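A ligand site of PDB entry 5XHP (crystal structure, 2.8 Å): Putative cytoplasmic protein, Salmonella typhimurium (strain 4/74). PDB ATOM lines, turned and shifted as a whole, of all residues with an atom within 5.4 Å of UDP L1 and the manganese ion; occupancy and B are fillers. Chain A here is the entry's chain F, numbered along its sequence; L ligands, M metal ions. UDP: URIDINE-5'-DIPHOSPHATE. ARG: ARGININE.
O of Phe 66 sits at hydrogen-bond distance from N3 of UDP L1 (2.8 Å). The backbone carbonyl oxygen (O) of Gln 64 lies within hydrogen-bond range of an oxygen (O2') of UDP L1. The side-chain carboxylate (OD2) of Asp 239 lies within salt-bridge range of a nitrogen (NH2) of ARG L2 (3.4 Å). An oxygen (O2) of UDP L1 sits at hydrogen-bond distance from the backbone NH (N) of Phe 66 (2.9 Å). O2A of UDP L1 sits at hydrogen-bond distance from OH of Tyr 88. O3' of UDP L1 sits at hydrogen-bond distance from N of Ala 240. A nitrogen (NH2) of ARG L2 is in hydrogen-bond range of the side-chain amide oxygen (OD1) of Asn 272 (2.8 Å). An oxygen (O2') of UDP L1 sits at hydrogen-bond distance from the side-chain hydroxyl (OH) of Tyr 237 (2.5 Å). OD1 of Asn 338 lies close to NH1 of ARG L2 (3.3 Å).
An oxygen (O1B) of UDP L1 lies close to a nitrogen (N) of ARG L2.
The side-chain hydroxyl (OH) of Tyr 88 lies within hydrogen-bond range of the side-chain amide nitrogen (ND2) of Asn 86, 3.1 Å away. OD1 of Asp 204 is in salt-bridge range of NH2 of Arg 207 (2.9 Å). The guanidinium group of Arg 207 lies within hydrogen-bond range of the backbone carbonyl oxygen of Asn 272, at 2.8 Å. The side-chain hydroxyl (OH) of Tyr 237 sits at hydrogen-bond distance from the side-chain carboxylate (OD1) of Asp 239 (3.2 Å). OD1 of Asp 239 is in salt-bridge range of NH1 of Arg 207. The side-chain hydroxyl of Tyr 237 is in hydrogen-bond range of the guanidinium group of Arg 207 (2.8 Å). The backbone carbonyl oxygen of Asp 241 is in hydrogen-bond range of the backbone NH of Thr 339, at 3.4 Å. The side-chain amide nitrogen of Gln 64 is in hydrogen-bond range of the backbone carbonyl oxygen of Phe 203, at 2.8 Å.
Residues that only touch UDP L1: Asp 239 (3.0 Å), Phe 203 (3.3 Å), Trp 65 (3.5 Å), Arg 207 (3.5 Å) and Asn 86 (3.8 Å). Hydrophobic or aromatic side chains that line UDP L1: Trp 65, Phe 66, Tyr 88, Phe 203, Tyr 237 and Ala 240. Of the 20 residues printed, 13 come within 4 Å of UDP L1. The nearest printed residue that does not touch UDP L1 is Arg 68 (4.1 Å).
The manganese ion is bound by the side-chain hydroxyl (OG) of Ser 340 (1.7 Å), an oxygen (O1B) of UDP L1 (2.2 Å), the side-chain amide oxygen (OD1) of Asn 338 (2.2 Å), an oxygen (O1A) of UDP L1 (2.2 Å) and the side-chain carboxylate (OD2) of Asp 241 (2.5 Å). The manganese ion has five donor atoms within binding distance.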
ATOM      1  N   GLN A  64       2.320 -14.719   1.782  1.00  0.00           N
ATOM      2  CA  GLN A  64       0.978 -14.254   2.082  1.00  0.00           C
ATOM      3  C   GLN A  64       0.184 -15.368   2.697  1.00  0.00           C
ATOM      4  O   GLN A  64       0.348 -16.520   2.287  1.00  0.00           O
ATOM      5  CB  GLN A  64       0.288 -13.780   0.807  1.00  0.00           C
ATOM      6  CG  GLN A  64      -1.230 -13.719   0.809  1.00  0.00           C
ATOM      7  CD  GLN A  64      -1.748 -13.124  -0.473  1.00  0.00           C
ATOM      8  OE1 GLN A  64      -1.214 -13.398  -1.540  1.00  0.00           O
ATOM      9  NE2 GLN A  64      -2.777 -12.303  -0.365  1.00  0.00           N
ATOM     10  N   TRP A  65      -0.653 -15.018   3.666  1.00  0.00           N
ATOM     11  CA  TRP A  65      -1.662 -15.957   4.138  1.00  0.00           C
ATOM     12  C   TRP A  65      -2.911 -15.194   4.511  1.00  0.00           C
ATOM     13  O   TRP A  65      -2.909 -14.393   5.426  1.00  0.00           O
ATOM     14  CB  TRP A  65      -1.178 -16.822   5.303  1.00  0.00           C
ATOM     15  CG  TRP A  65      -2.170 -17.902   5.633  1.00  0.00           C
ATOM     16  CD1 TRP A  65      -3.022 -17.927   6.682  1.00  0.00           C
ATOM     17  CD2 TRP A  65      -2.425 -19.108   4.888  1.00  0.00           C
ATOM     18  NE1 TRP A  65      -3.782 -19.064   6.666  1.00  0.00           N
ATOM     19  CE2 TRP A  65      -3.440 -19.806   5.557  1.00  0.00           C
ATOM     20  CE3 TRP A  65      -1.885 -19.665   3.717  1.00  0.00           C
ATOM     21  CZ2 TRP A  65      -3.940 -21.041   5.111  1.00  0.00           C
ATOM     22  CZ3 TRP A  65      -2.392 -20.892   3.269  1.00  0.00           C
ATOM     23  CH2 TRP A  65      -3.410 -21.570   3.969  1.00  0.00           C
ATOM     24  N   PHE A  66      -3.960 -15.436   3.740  1.00  0.00           N
ATOM     25  CA  PHE A  66      -5.277 -14.907   3.985  1.00  0.00           C
ATOM     26  C   PHE A  66      -6.053 -16.092   4.501  1.00  0.00           C
ATOM     27  O   PHE A  66      -6.252 -17.070   3.763  1.00  0.00           O
ATOM     28  CB  PHE A  66      -5.852 -14.340   2.695  1.00  0.00           C
ATOM     29  CG  PHE A  66      -5.455 -12.895   2.404  1.00  0.00           C
ATOM     30  CD1 PHE A  66      -4.317 -12.321   2.962  1.00  0.00           C
ATOM     31  CD2 PHE A  66      -6.230 -12.117   1.543  1.00  0.00           C
ATOM     32  CE1 PHE A  66      -3.983 -11.004   2.682  1.00  0.00           C
ATOM     33  CE2 PHE A  66      -5.902 -10.807   1.260  1.00  0.00           C
ATOM     34  CZ  PHE A  66      -4.780 -10.254   1.845  1.00  0.00           C
ATOM     35  N   GLU A  67      -6.393 -16.063   5.778  1.00  0.00           N
ATOM     36  CA  GLU A  67      -6.923 -17.225   6.384  1.00  0.00           C
ATOM     37  C   GLU A  67      -8.363 -17.008   6.464  1.00  0.00           C
ATOM     38  O   GLU A  67      -8.841 -16.112   7.160  1.00  0.00           O
ATOM     39  CB  GLU A  67      -6.405 -17.460   7.771  1.00  0.00           C
ATOM     40  CG  GLU A  67      -7.058 -18.679   8.390  1.00  0.00           C
ATOM     41  CD  GLU A  67      -6.820 -19.952   7.594  1.00  0.00           C
ATOM     42  OE1 GLU A  67      -7.792 -20.708   7.352  1.00  0.00           O
ATOM     43  OE2 GLU A  67      -5.671 -20.200   7.220  1.00  0.00           O
ATOM     44  N   ARG A  68      -9.031 -17.905   5.794  1.00  0.00           N
ATOM     45  CA  ARG A  68     -10.453 -17.901   5.638  1.00  0.00           C
ATOM     46  C   ARG A  68     -11.092 -18.072   7.018  1.00  0.00           C
ATOM     47  O   ARG A  68     -12.031 -17.370   7.376  1.00  0.00           O
ATOM     48  CB  ARG A  68     -10.825 -19.001   4.634  1.00  0.00           C
ATOM     49  CG  ARG A  68     -10.217 -18.788   3.212  1.00  0.00           C
ATOM     50  CD  ARG A  68     -10.393 -19.922   2.177  1.00  0.00           C
ATOM     51  NE  ARG A  68      -9.847 -19.603   0.830  1.00  0.00           N
ATOM     52  CZ  ARG A  68      -9.745 -20.467  -0.199  1.00  0.00           C
ATOM     53  NH1 ARG A  68     -10.137 -21.735  -0.085  1.00  0.00           N
ATOM     54  NH2 ARG A  68      -9.228 -20.062  -1.366  1.00  0.00           N
ATOM     55  N   ASN A  86       0.737 -29.392   3.598  1.00  0.00           N
ATOM     56  CA  ASN A  86       1.337 -28.080   3.436  1.00  0.00           C
ATOM     57  C   ASN A  86       1.660 -27.566   4.813  1.00  0.00           C
ATOM     58  O   ASN A  86       0.779 -27.125   5.526  1.00  0.00           O
ATOM     59  CB  ASN A  86       0.399 -27.083   2.732  1.00  0.00           C
ATOM     60  CG  ASN A  86       0.209 -27.399   1.262  1.00  0.00           C
ATOM     61  OD1 ASN A  86       1.030 -28.045   0.624  1.00  0.00           O
ATOM     62  ND2 ASN A  86      -0.889 -26.891   0.716  1.00  0.00           N
ATOM     63  N   TYR A  88       2.922 -24.805   5.927  1.00  0.00           N
ATOM     64  CA  TYR A  88       3.359 -23.552   5.354  1.00  0.00           C
ATOM     65  C   TYR A  88       4.167 -22.668   6.279  1.00  0.00           C
ATOM     66  O   TYR A  88       5.099 -21.976   5.845  1.00  0.00           O
ATOM     67  CB  TYR A  88       2.180 -22.825   4.709  1.00  0.00           C
ATOM     68  CG  TYR A  88       1.867 -23.388   3.325  1.00  0.00           C
ATOM     69  CD1 TYR A  88       2.834 -24.119   2.608  1.00  0.00           C
ATOM     70  CD2 TYR A  88       0.639 -23.157   2.706  1.00  0.00           C
ATOM     71  CE1 TYR A  88       2.575 -24.625   1.378  1.00  0.00           C
ATOM     72  CE2 TYR A  88       0.376 -23.663   1.443  1.00  0.00           C
ATOM     73  CZ  TYR A  88       1.367 -24.379   0.787  1.00  0.00           C
ATOM     74  OH  TYR A  88       1.138 -24.885  -0.444  1.00  0.00           O
ATOM     75  N   PHE A 203      -7.353 -13.263  -1.891  1.00  0.00           N
ATOM     76  CA  PHE A 203      -5.871 -13.111  -1.695  1.00  0.00           C
ATOM     77  C   PHE A 203      -5.059 -12.910  -2.966  1.00  0.00           C
ATOM     78  O   PHE A 203      -3.960 -12.372  -2.904  1.00  0.00           O
ATOM     79  CB  PHE A 203      -5.245 -14.237  -0.851  1.00  0.00           C
ATOM     80  CG  PHE A 203      -5.721 -15.626  -1.184  1.00  0.00           C
ATOM     81  CD1 PHE A 203      -6.842 -16.156  -0.560  1.00  0.00           C
ATOM     82  CD2 PHE A 203      -5.019 -16.422  -2.071  1.00  0.00           C
ATOM     83  CE1 PHE A 203      -7.278 -17.446  -0.838  1.00  0.00           C
ATOM     84  CE2 PHE A 203      -5.442 -17.720  -2.366  1.00  0.00           C
ATOM     85  CZ  PHE A 203      -6.569 -18.228  -1.744  1.00  0.00           C
ATOM     86  N   ASP A 204      -5.566 -13.368  -4.098  1.00  0.00           N
ATOM     87  CA  ASP A 204      -4.884 -13.104  -5.359  1.00  0.00           C
ATOM     88  C   ASP A 204      -5.099 -11.685  -5.849  1.00  0.00           C
ATOM     89  O   ASP A 204      -4.220 -11.143  -6.510  1.00  0.00           O
ATOM     90  CB  ASP A 204      -5.305 -14.113  -6.421  1.00  0.00           C
ATOM     91  CG  ASP A 204      -4.853 -15.538  -6.085  1.00  0.00           C
ATOM     92  OD1 ASP A 204      -3.959 -15.714  -5.217  1.00  0.00           O
ATOM     93  OD2 ASP A 204      -5.407 -16.476  -6.696  1.00  0.00           O
ATOM     94  N   ARG A 207      -2.929  -9.411  -3.399  1.00  0.00           N
ATOM     95  CA  ARG A 207      -1.542  -9.664  -3.706  1.00  0.00           C
ATOM     96  C   ARG A 207      -1.074  -8.602  -4.668  1.00  0.00           C
ATOM     97  O   ARG A 207      -0.160  -7.838  -4.362  1.00  0.00           O
ATOM     98  CB  ARG A 207      -1.358 -11.042  -4.309  1.00  0.00           C
ATOM     99  CG  ARG A 207       0.101 -11.436  -4.467  1.00  0.00           C
ATOM    100  CD  ARG A 207       0.204 -12.858  -4.960  1.00  0.00           C
ATOM    101  NE  ARG A 207      -0.599 -13.745  -4.138  1.00  0.00           N
ATOM    102  CZ  ARG A 207      -0.804 -15.041  -4.372  1.00  0.00           C
ATOM    103  NH1 ARG A 207      -0.206 -15.661  -5.377  1.00  0.00           N
ATOM    104  NH2 ARG A 207      -1.574 -15.724  -3.540  1.00  0.00           N
ATOM    105  N   TYR A 237       7.087 -11.736  -4.157  1.00  0.00           N
ATOM    106  CA  TYR A 237       6.075 -12.569  -3.518  1.00  0.00           C
ATOM    107  C   TYR A 237       6.407 -14.045  -3.705  1.00  0.00           C
ATOM    108  O   TYR A 237       7.041 -14.417  -4.666  1.00  0.00           O
ATOM    109  CB  TYR A 237       4.679 -12.268  -4.034  1.00  0.00           C
ATOM    110  CG  TYR A 237       3.670 -13.313  -3.625  1.00  0.00           C
ATOM    111  CD1 TYR A 237       3.224 -13.391  -2.319  1.00  0.00           C
ATOM    112  CD2 TYR A 237       3.195 -14.237  -4.526  1.00  0.00           C
ATOM    113  CE1 TYR A 237       2.337 -14.344  -1.945  1.00  0.00           C
ATOM    114  CE2 TYR A 237       2.301 -15.183  -4.154  1.00  0.00           C
ATOM    115  CZ  TYR A 237       1.868 -15.240  -2.865  1.00  0.00           C
ATOM    116  OH  TYR A 237       0.970 -16.207  -2.504  1.00  0.00           O
ATOM    117  N   LEU A 238       6.023 -14.859  -2.757  1.00  0.00           N
ATOM    118  CA  LEU A 238       6.189 -16.279  -2.893  1.00  0.00           C
ATOM    119  C   LEU A 238       4.987 -17.007  -2.379  1.00  0.00           C
ATOM    120  O   LEU A 238       4.435 -16.670  -1.328  1.00  0.00           O
ATOM    121  CB  LEU A 238       7.396 -16.722  -2.113  1.00  0.00           C
ATOM    122  CG  LEU A 238       8.700 -16.071  -2.594  1.00  0.00           C
ATOM    123  CD1 LEU A 238       9.642 -15.801  -1.447  1.00  0.00           C
ATOM    124  CD2 LEU A 238       9.344 -16.903  -3.689  1.00  0.00           C
ATOM    125  N   ASP A 239       4.575 -18.044  -3.102  1.00  0.00           N
ATOM    126  CA  ASP A 239       3.567 -18.940  -2.588  1.00  0.00           C
ATOM    127  C   ASP A 239       4.266 -19.563  -1.405  1.00  0.00           C
ATOM    128  O   ASP A 239       5.466 -19.746  -1.457  1.00  0.00           O
ATOM    129  CB  ASP A 239       3.167 -20.006  -3.622  1.00  0.00           C
ATOM    130  CG  ASP A 239       2.372 -19.440  -4.784  1.00  0.00           C
ATOM    131  OD1 ASP A 239       1.867 -18.326  -4.716  1.00  0.00           O
ATOM    132  OD2 ASP A 239       2.273 -20.129  -5.815  1.00  0.00           O
ATOM    133  N   ALA A 240       3.552 -19.877  -0.343  1.00  0.00           N
ATOM    134  CA  ALA A 240       4.211 -20.358   0.869  1.00  0.00           C
ATOM    135  C   ALA A 240       4.941 -21.641   0.569  1.00  0.00           C
ATOM    136  O   ALA A 240       5.830 -22.015   1.320  1.00  0.00           O
ATOM    137  CB  ALA A 240       3.187 -20.596   1.945  1.00  0.00           C
ATOM    138  N   ASP A 241       4.527 -22.296  -0.522  1.00  0.00           N
ATOM    139  CA  ASP A 241       5.068 -23.594  -0.925  1.00  0.00           C
ATOM    140  C   ASP A 241       6.257 -23.588  -1.885  1.00  0.00           C
ATOM    141  O   ASP A 241       6.786 -24.653  -2.187  1.00  0.00           O
ATOM    142  CB  ASP A 241       3.983 -24.529  -1.477  1.00  0.00           C
ATOM    143  CG  ASP A 241       3.255 -23.977  -2.659  1.00  0.00           C
ATOM    144  OD1 ASP A 241       2.939 -22.785  -2.698  1.00  0.00           O
ATOM    145  OD2 ASP A 241       2.947 -24.780  -3.548  1.00  0.00           O
ATOM    146  N   ASN A 272       0.575 -17.172 -10.570  1.00  0.00           N
ATOM    147  CA  ASN A 272       0.696 -16.158  -9.521  1.00  0.00           C
ATOM    148  C   ASN A 272       1.530 -16.688  -8.368  1.00  0.00           C
ATOM    149  O   ASN A 272       1.708 -16.020  -7.374  1.00  0.00           O
ATOM    150  CB  ASN A 272      -0.678 -15.742  -9.052  1.00  0.00           C
ATOM    151  CG  ASN A 272      -1.392 -16.834  -8.296  1.00  0.00           C
ATOM    152  OD1 ASN A 272      -0.858 -17.934  -8.081  1.00  0.00           O
ATOM    153  ND2 ASN A 272      -2.609 -16.538  -7.871  1.00  0.00           N
ATOM    154  N   ASN A 338       6.590 -24.415  -6.424  1.00  0.00           N
ATOM    155  CA  ASN A 338       5.171 -24.834  -6.348  1.00  0.00           C
ATOM    156  C   ASN A 338       5.068 -26.284  -5.930  1.00  0.00           C
ATOM    157  O   ASN A 338       4.644 -27.158  -6.688  1.00  0.00           O
ATOM    158  CB  ASN A 338       4.467 -24.566  -7.691  1.00  0.00           C
ATOM    159  CG  ASN A 338       3.066 -25.169  -7.756  1.00  0.00           C
ATOM    160  OD1 ASN A 338       2.223 -24.940  -6.884  1.00  0.00           O
ATOM    161  ND2 ASN A 338       2.813 -25.943  -8.816  1.00  0.00           N
ATOM    162  N   THR A 339       5.506 -26.547  -4.705  1.00  0.00           N
ATOM    163  CA  THR A 339       5.509 -27.904  -4.137  1.00  0.00           C
ATOM    164  C   THR A 339       4.142 -28.407  -3.623  1.00  0.00           C
ATOM    165  O   THR A 339       4.044 -29.567  -3.204  1.00  0.00           O
ATOM    166  CB  THR A 339       6.570 -28.043  -3.025  1.00  0.00           C
ATOM    167  OG1 THR A 339       6.418 -26.996  -2.076  1.00  0.00           O
ATOM    168  CG2 THR A 339       7.957 -27.993  -3.637  1.00  0.00           C
ATOM    169  N   SER A 340       3.105 -27.558  -3.676  1.00  0.00           N
ATOM    170  CA  SER A 340       1.732 -27.977  -3.375  1.00  0.00           C
ATOM    171  C   SER A 340       1.131 -28.959  -4.390  1.00  0.00           C
ATOM    172  O   SER A 340       0.232 -29.706  -4.051  1.00  0.00           O
ATOM    173  CB  SER A 340       0.791 -26.767  -3.207  1.00  0.00           C
ATOM    174  OG  SER A 340       0.962 -25.770  -4.192  1.00  0.00           O
ATOM    175  N   SER A 341       1.643 -28.979  -5.622  1.00  0.00           N
ATOM    176  CA  SER A 341       1.194 -30.009  -6.577  1.00  0.00           C
ATOM    177  C   SER A 341       1.595 -31.441  -6.154  1.00  0.00           C
ATOM    178  O   SER A 341       1.077 -32.414  -6.711  1.00  0.00           O
ATOM    179  CB  SER A 341       1.641 -29.705  -8.030  1.00  0.00           C
ATOM    180  OG  SER A 341       2.972 -29.236  -8.135  1.00  0.00           O
HETATM  181  N1  UDP L   1      -3.386 -18.833  -0.018  1.00  0.00           N
HETATM  182  C2  UDP L   1      -3.860 -18.007   1.038  1.00  0.00           C
HETATM  183  N3  UDP L   1      -4.796 -18.464   1.870  1.00  0.00           N
HETATM  184  C4  UDP L   1      -5.302 -19.691   1.694  1.00  0.00           C
HETATM  185  C5  UDP L   1      -4.863 -20.525   0.680  1.00  0.00           C
HETATM  186  C6  UDP L   1      -3.889 -20.067  -0.181  1.00  0.00           C
HETATM  187  O2  UDP L   1      -3.399 -16.851   1.219  1.00  0.00           O
HETATM  188  O4  UDP L   1      -6.173 -20.106   2.463  1.00  0.00           O
HETATM  189  C1' UDP L   1      -2.352 -18.347  -0.923  1.00  0.00           C
HETATM  190  C2' UDP L   1      -1.011 -18.337  -0.246  1.00  0.00           C
HETATM  191  O2' UDP L   1      -0.346 -17.103  -0.535  1.00  0.00           O
HETATM  192  C3' UDP L   1      -0.266 -19.458  -0.888  1.00  0.00           C
HETATM  193  C4' UDP L   1      -0.843 -19.471  -2.294  1.00  0.00           C
HETATM  194  O4' UDP L   1      -2.230 -19.162  -2.082  1.00  0.00           O
HETATM  195  O3' UDP L   1       1.140 -19.229  -0.852  1.00  0.00           O
HETATM  196  C5' UDP L   1      -0.637 -20.808  -3.016  1.00  0.00           C
HETATM  197  O5' UDP L   1      -1.620 -21.754  -2.600  1.00  0.00           O
HETATM  198  PA  UDP L   1      -1.438 -23.344  -2.783  1.00  0.00           P
HETATM  199  O1A UDP L   1      -0.049 -23.633  -3.299  1.00  0.00           O
HETATM  200  O2A UDP L   1      -1.836 -23.974  -1.472  1.00  0.00           O
HETATM  201  O3A UDP L   1      -2.621 -23.665  -3.850  1.00  0.00           O
HETATM  202  PB  UDP L   1      -2.449 -23.702  -5.455  1.00  0.00           P
HETATM  203  O1B UDP L   1      -1.014 -24.061  -5.747  1.00  0.00           O
HETATM  204  O2B UDP L   1      -3.460 -24.784  -5.752  1.00  0.00           O
HETATM  205  O3B UDP L   1      -2.786 -22.348  -6.006  1.00  0.00           O
HETATM  206  N   ARG L   2      -1.083 -26.695  -7.536  1.00  0.00           N
HETATM  207  CA  ARG L   2      -1.200 -26.685  -9.056  1.00  0.00           C
HETATM  208  C   ARG L   2      -1.299 -28.108  -9.614  1.00  0.00           C
HETATM  209  O   ARG L   2      -0.449 -28.584 -10.390  1.00  0.00           O
HETATM  210  CB  ARG L   2      -0.029 -25.936  -9.727  1.00  0.00           C
HETATM  211  CG  ARG L   2      -0.231 -24.445  -9.940  1.00  0.00           C
HETATM  212  CD  ARG L   2      -0.531 -23.745  -8.639  1.00  0.00           C
HETATM  213  NE  ARG L   2      -0.450 -22.309  -8.717  1.00  0.00           N
HETATM  214  CZ  ARG L   2       0.668 -21.580  -8.649  1.00  0.00           C
HETATM  215  NH1 ARG L   2       1.882 -22.138  -8.529  1.00  0.00           N
HETATM  216  NH2 ARG L   2       0.567 -20.280  -8.734  1.00  0.00           N
HETATM  217  OXT ARG L   2      -2.256 -28.813  -9.284  1.00  0.00           O
HETATM  218 MN    MN M   1       1.076 -24.336  -5.101  1.00  0.00          MN
